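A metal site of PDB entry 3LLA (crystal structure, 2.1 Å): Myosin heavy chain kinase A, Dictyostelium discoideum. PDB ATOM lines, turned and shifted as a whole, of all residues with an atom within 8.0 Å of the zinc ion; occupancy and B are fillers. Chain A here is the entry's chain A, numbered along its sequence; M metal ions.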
ATOM      1  N   SER A 201       5.542  14.629 -18.347  1.00  0.00           N
ATOM      2  CA  SER A 201       4.779  15.776 -18.831  1.00  0.00           C
ATOM      3  C   SER A 201       4.217  16.688 -17.724  1.00  0.00           C
ATOM      4  O   SER A 201       4.141  17.912 -17.898  1.00  0.00           O
ATOM      5  CB  SER A 201       3.659  15.314 -19.747  1.00  0.00           C
ATOM      6  OG  SER A 201       4.202  14.673 -20.895  1.00  0.00           O
ATOM      7  N   GLN A 204       6.447  19.648 -16.350  1.00  0.00           N
ATOM      8  CA  GLN A 204       6.576  20.698 -17.348  1.00  0.00           C
ATOM      9  C   GLN A 204       5.270  21.433 -17.552  1.00  0.00           C
ATOM     10  O   GLN A 204       5.266  22.654 -17.773  1.00  0.00           O
ATOM     11  CB  GLN A 204       7.079  20.145 -18.700  1.00  0.00           C
ATOM     12  CG  GLN A 204       8.337  19.259 -18.589  1.00  0.00           C
ATOM     13  CD  GLN A 204       9.469  19.947 -17.845  1.00  0.00           C
ATOM     14  OE1 GLN A 204       9.648  21.164 -17.951  1.00  0.00           O
ATOM     15  NE2 GLN A 204      10.247  19.169 -17.091  1.00  0.00           N
ATOM     16  N   ALA A 205       4.150  20.713 -17.500  1.00  0.00           N
ATOM     17  CA  ALA A 205       2.857  21.347 -17.669  1.00  0.00           C
ATOM     18  C   ALA A 205       2.486  22.198 -16.460  1.00  0.00           C
ATOM     19  O   ALA A 205       1.778  23.193 -16.600  1.00  0.00           O
ATOM     20  CB  ALA A 205       1.764  20.326 -17.945  1.00  0.00           C
ATOM     21  N   PHE A 206       2.946  21.793 -15.285  1.00  0.00           N
ATOM     22  CA  PHE A 206       2.745  22.563 -14.051  1.00  0.00           C
ATOM     23  C   PHE A 206       3.503  23.905 -14.097  1.00  0.00           C
ATOM     24  O   PHE A 206       2.934  24.949 -13.797  1.00  0.00           O
ATOM     25  CB  PHE A 206       3.159  21.757 -12.816  1.00  0.00           C
ATOM     26  CG  PHE A 206       3.170  22.580 -11.558  1.00  0.00           C
ATOM     27  CD1 PHE A 206       1.976  22.942 -10.935  1.00  0.00           C
ATOM     28  CD2 PHE A 206       4.369  23.040 -11.025  1.00  0.00           C
ATOM     29  CE1 PHE A 206       1.999  23.733  -9.780  1.00  0.00           C
ATOM     30  CE2 PHE A 206       4.389  23.823  -9.881  1.00  0.00           C
ATOM     31  CZ  PHE A 206       3.202  24.158  -9.249  1.00  0.00           C
ATOM     32  N   SER A 207       4.770  23.851 -14.505  1.00  0.00           N
ATOM     33  CA  SER A 207       5.552  25.054 -14.712  1.00  0.00           C
ATOM     34  C   SER A 207       4.831  26.007 -15.665  1.00  0.00           C
ATOM     35  O   SER A 207       4.595  27.194 -15.330  1.00  0.00           O
ATOM     36  CB  SER A 207       6.963  24.716 -15.209  1.00  0.00           C
ATOM     37  OG  SER A 207       7.712  24.020 -14.208  1.00  0.00           O
ATOM     38  N   HIS A 208       4.439  25.489 -16.836  1.00  0.00           N
ATOM     39  CA  HIS A 208       3.680  26.292 -17.789  1.00  0.00           C
ATOM     40  C   HIS A 208       2.375  26.847 -17.150  1.00  0.00           C
ATOM     41  O   HIS A 208       2.058  28.051 -17.279  1.00  0.00           O
ATOM     42  CB  HIS A 208       3.367  25.482 -19.093  1.00  0.00           C
ATOM     43  CG  HIS A 208       2.756  26.319 -20.178  1.00  0.00           C
ATOM     44  ND1 HIS A 208       2.480  25.829 -21.438  1.00  0.00           N
ATOM     45  CD2 HIS A 208       2.365  27.614 -20.191  1.00  0.00           C
ATOM     46  CE1 HIS A 208       1.926  26.778 -22.165  1.00  0.00           C
ATOM     47  NE2 HIS A 208       1.857  27.875 -21.439  1.00  0.00           N
ATOM     48  N   PHE A 209       1.613  25.988 -16.480  1.00  0.00           N
ATOM     49  CA  PHE A 209       0.377  26.424 -15.788  1.00  0.00           C
ATOM     50  C   PHE A 209       0.637  27.598 -14.830  1.00  0.00           C
ATOM     51  O   PHE A 209      -0.116  28.567 -14.827  1.00  0.00           O
ATOM     52  CB  PHE A 209      -0.215  25.227 -15.024  1.00  0.00           C
ATOM     53  CG  PHE A 209      -1.426  25.533 -14.164  1.00  0.00           C
ATOM     54  CD1 PHE A 209      -2.710  25.365 -14.678  1.00  0.00           C
ATOM     55  CD2 PHE A 209      -1.282  25.914 -12.827  1.00  0.00           C
ATOM     56  CE1 PHE A 209      -3.836  25.598 -13.880  1.00  0.00           C
ATOM     57  CE2 PHE A 209      -2.387  26.146 -12.015  1.00  0.00           C
ATOM     58  CZ  PHE A 209      -3.683  25.997 -12.539  1.00  0.00           C
ATOM     59  N   GLU A 212       1.149  30.867 -16.982  1.00  0.00           N
ATOM     60  CA  GLU A 212      -0.048  31.402 -17.602  1.00  0.00           C
ATOM     61  C   GLU A 212      -1.092  31.871 -16.584  1.00  0.00           C
ATOM     62  O   GLU A 212      -1.650  32.965 -16.728  1.00  0.00           O
ATOM     63  CB  GLU A 212      -0.662  30.409 -18.601  1.00  0.00           C
ATOM     64  CG  GLU A 212      -2.016  30.871 -19.155  1.00  0.00           C
ATOM     65  CD  GLU A 212      -2.505  30.108 -20.397  1.00  0.00           C
ATOM     66  OE1 GLU A 212      -1.684  29.599 -21.174  1.00  0.00           O
ATOM     67  OE2 GLU A 212      -3.736  30.058 -20.573  1.00  0.00           O
ATOM     68  N   PHE A 256      13.068  29.209 -19.495  1.00  0.00           N
ATOM     69  CA  PHE A 256      12.014  28.189 -19.497  1.00  0.00           C
ATOM     70  C   PHE A 256      11.246  28.192 -20.817  1.00  0.00           C
ATOM     71  O   PHE A 256      10.944  27.130 -21.345  1.00  0.00           O
ATOM     72  CB  PHE A 256      11.018  28.342 -18.324  1.00  0.00           C
ATOM     73  CG  PHE A 256       9.910  27.341 -18.355  1.00  0.00           C
ATOM     74  CD1 PHE A 256      10.070  26.087 -17.780  1.00  0.00           C
ATOM     75  CD2 PHE A 256       8.718  27.637 -19.026  1.00  0.00           C
ATOM     76  CE1 PHE A 256       9.060  25.145 -17.829  1.00  0.00           C
ATOM     77  CE2 PHE A 256       7.686  26.694 -19.078  1.00  0.00           C
ATOM     78  CZ  PHE A 256       7.854  25.443 -18.481  1.00  0.00           C
ATOM     79  N   HIS A 260      10.584  24.889 -23.456  1.00  0.00           N
ATOM     80  CA  HIS A 260       9.266  24.251 -23.230  1.00  0.00           C
ATOM     81  C   HIS A 260       8.649  23.782 -24.542  1.00  0.00           C
ATOM     82  O   HIS A 260       8.553  24.539 -25.506  1.00  0.00           O
ATOM     83  CB  HIS A 260       8.254  25.165 -22.485  1.00  0.00           C
ATOM     84  CG  HIS A 260       6.940  24.497 -22.158  1.00  0.00           C
ATOM     85  ND1 HIS A 260       6.828  23.484 -21.226  1.00  0.00           N
ATOM     86  CD2 HIS A 260       5.672  24.702 -22.616  1.00  0.00           C
ATOM     87  CE1 HIS A 260       5.555  23.113 -21.111  1.00  0.00           C
ATOM     88  NE2 HIS A 260       4.839  23.833 -21.950  1.00  0.00           N
ATOM     89  N   LYS A 261       8.248  22.517 -24.534  1.00  0.00           N
ATOM     90  CA  LYS A 261       7.392  21.941 -25.564  1.00  0.00           C
ATOM     91  C   LYS A 261       6.111  21.571 -24.858  1.00  0.00           C
ATOM     92  O   LYS A 261       6.138  20.818 -23.866  1.00  0.00           O
ATOM     93  CB  LYS A 261       8.033  20.664 -26.125  1.00  0.00           C
ATOM     94  CG  LYS A 261       9.256  20.881 -27.018  1.00  0.00           C
ATOM     95  CD  LYS A 261       9.436  19.686 -27.987  1.00  0.00           C
ATOM     96  CE  LYS A 261       8.470  19.781 -29.183  1.00  0.00           C
ATOM     97  NZ  LYS A 261       8.273  18.482 -29.906  1.00  0.00           N
ATOM     98  N   CYS A 262       4.991  22.100 -25.331  1.00  0.00           N
ATOM     99  CA  CYS A 262       3.694  21.779 -24.736  1.00  0.00           C
ATOM    100  C   CYS A 262       3.369  20.298 -24.967  1.00  0.00           C
ATOM    101  O   CYS A 262       3.691  19.742 -26.017  1.00  0.00           O
ATOM    102  CB  CYS A 262       2.584  22.674 -25.288  1.00  0.00           C
ATOM    103  SG  CYS A 262       2.385  24.294 -24.469  1.00  0.00           S
ATOM    104  N   ASN A 263       2.750  19.672 -23.964  1.00  0.00           N
ATOM    105  CA  ASN A 263       2.435  18.244 -24.015  1.00  0.00           C
ATOM    106  C   ASN A 263       0.943  18.054 -23.793  1.00  0.00           C
ATOM    107  O   ASN A 263       0.180  19.034 -23.761  1.00  0.00           O
ATOM    108  CB  ASN A 263       3.226  17.517 -22.948  1.00  0.00           C
ATOM    109  CG  ASN A 263       2.979  18.079 -21.556  1.00  0.00           C
ATOM    110  OD1 ASN A 263       1.827  18.212 -21.140  1.00  0.00           O
ATOM    111  ND2 ASN A 263       4.041  18.449 -20.853  1.00  0.00           N
ATOM    112  N   ALA A 264       0.513  16.806 -23.615  1.00  0.00           N
ATOM    113  CA  ALA A 264      -0.922  16.503 -23.464  1.00  0.00           C
ATOM    114  C   ALA A 264      -1.522  17.106 -22.208  1.00  0.00           C
ATOM    115  O   ALA A 264      -2.705  17.490 -22.194  1.00  0.00           O
ATOM    116  CB  ALA A 264      -1.171  14.986 -23.500  1.00  0.00           C
ATOM    117  N   VAL A 265      -0.733  17.160 -21.145  1.00  0.00           N
ATOM    118  CA  VAL A 265      -1.180  17.818 -19.905  1.00  0.00           C
ATOM    119  C   VAL A 265      -1.408  19.327 -20.165  1.00  0.00           C
ATOM    120  O   VAL A 265      -2.446  19.856 -19.825  1.00  0.00           O
ATOM    121  CB  VAL A 265      -0.229  17.560 -18.685  1.00  0.00           C
ATOM    122  CG1 VAL A 265      -0.932  17.959 -17.395  1.00  0.00           C
ATOM    123  CG2 VAL A 265       0.136  16.096 -18.600  1.00  0.00           C
ATOM    124  N   CYS A 266      -0.465  20.010 -20.816  1.00  0.00           N
ATOM    125  CA  CYS A 266      -0.712  21.417 -21.210  1.00  0.00           C
ATOM    126  C   CYS A 266      -2.006  21.588 -21.982  1.00  0.00           C
ATOM    127  O   CYS A 266      -2.819  22.477 -21.681  1.00  0.00           O
ATOM    128  CB  CYS A 266       0.434  21.974 -22.058  1.00  0.00           C
ATOM    129  SG  CYS A 266       2.007  21.918 -21.274  1.00  0.00           S
ATOM    130  N   ALA A 267      -2.207  20.730 -22.983  1.00  0.00           N
ATOM    131  CA  ALA A 267      -3.385  20.816 -23.832  1.00  0.00           C
ATOM    132  C   ALA A 267      -4.654  20.547 -23.034  1.00  0.00           C
ATOM    133  O   ALA A 267      -5.666  21.229 -23.197  1.00  0.00           O
ATOM    134  CB  ALA A 267      -3.260  19.831 -25.028  1.00  0.00           C
ATOM    135  N   LEU A 271      -3.947  25.405 -21.896  1.00  0.00           N
ATOM    136  CA  LEU A 271      -2.873  26.378 -21.873  1.00  0.00           C
ATOM    137  C   LEU A 271      -2.489  26.784 -23.297  1.00  0.00           C
ATOM    138  O   LEU A 271      -2.470  25.965 -24.213  1.00  0.00           O
ATOM    139  CB  LEU A 271      -1.644  25.802 -21.159  1.00  0.00           C
ATOM    140  CG  LEU A 271      -1.835  25.262 -19.730  1.00  0.00           C
ATOM    141  CD1 LEU A 271      -0.529  24.694 -19.205  1.00  0.00           C
ATOM    142  CD2 LEU A 271      -2.396  26.336 -18.783  1.00  0.00           C
ATOM    143  N   ASP A 272      -2.167  28.069 -23.462  1.00  0.00           N
ATOM    144  CA  ASP A 272      -1.843  28.616 -24.773  1.00  0.00           C
ATOM    145  C   ASP A 272      -0.459  28.146 -25.215  1.00  0.00           C
ATOM    146  O   ASP A 272       0.511  28.355 -24.492  1.00  0.00           O
ATOM    147  CB  ASP A 272      -1.903  30.149 -24.723  1.00  0.00           C
ATOM    148  CG  ASP A 272      -2.087  30.785 -26.102  1.00  0.00           C
ATOM    149  OD1 ASP A 272      -1.472  30.296 -27.090  1.00  0.00           O
ATOM    150  OD2 ASP A 272      -2.826  31.798 -26.195  1.00  0.00           O
ATOM    151  N   VAL A 273      -0.367  27.517 -26.386  1.00  0.00           N
ATOM    152  CA  VAL A 273       0.940  27.164 -26.976  1.00  0.00           C
ATOM    153  C   VAL A 273       1.854  28.386 -27.187  1.00  0.00           C
ATOM    154  O   VAL A 273       3.075  28.241 -27.275  1.00  0.00           O
ATOM    155  CB  VAL A 273       0.811  26.376 -28.315  1.00  0.00           C
ATOM    156  CG1 VAL A 273       0.275  24.975 -28.069  1.00  0.00           C
ATOM    157  CG2 VAL A 273      -0.062  27.132 -29.335  1.00  0.00           C
ATOM    158  N   LYS A 274       1.257  29.578 -27.279  1.00  0.00           N
ATOM    159  CA  LYS A 274       2.043  30.832 -27.276  1.00  0.00           C
ATOM    160  C   LYS A 274       2.283  31.275 -25.844  1.00  0.00           C
ATOM    161  O   LYS A 274       1.311  31.512 -25.088  1.00  0.00           O
ATOM    162  CB  LYS A 274       1.314  31.966 -28.031  1.00  0.00           C
ATOM    163  CG  LYS A 274       0.776  31.609 -29.430  1.00  0.00           C
ATOM    164  CD  LYS A 274       1.868  31.119 -30.390  1.00  0.00           C
ATOM    165  CE  LYS A 274       2.960  32.164 -30.633  1.00  0.00           C
ATOM    166  NZ  LYS A 274       3.850  31.762 -31.756  1.00  0.00           N
ATOM    167  N   LEU A 275       3.548  31.371 -25.442  1.00  0.00           N
ATOM    168  CA  LEU A 275       3.888  31.898 -24.117  1.00  0.00           C
ATOM    169  C   LEU A 275       4.357  33.354 -24.187  1.00  0.00           C
ATOM    170  O   LEU A 275       3.721  34.249 -23.617  1.00  0.00           O
ATOM    171  CB  LEU A 275       4.941  31.017 -23.432  1.00  0.00           C
ATOM    172  CG  LEU A 275       4.477  29.688 -22.828  1.00  0.00           C
ATOM    173  CD1 LEU A 275       4.585  28.565 -23.835  1.00  0.00           C
ATOM    174  CD2 LEU A 275       5.262  29.354 -21.574  1.00  0.00           C
HETATM  175 ZN    ZN M   1       2.954  23.908 -22.148  1.00  0.00          ZN
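A ring nitrogen (NE2) of His 208 lies close to the backbone carbonyl oxygen (O) of Asp 272. N of Cys 266 sits at hydrogen-bond distance from OD1 of Asn 263 (2.9 Å). N of Leu 271 is in hydrogen-bond range of O of Cys 266 (3.1 Å).
Of the 22 residues printed, 4 come within 4 Å of the zinc ion. The nearest printed residue that does not touch the zinc ion is Asn 263 (4.6 Å).
The zinc ion is bound by a ring nitrogen (NE2) of His 260 (1.9 Å), a ring nitrogen (ND1) of His 208 (2.1 Å), the side-chain sulfur of Cys 266 (2.4 Å) and the side-chain sulfur of Cys 262 (2.4 Å).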
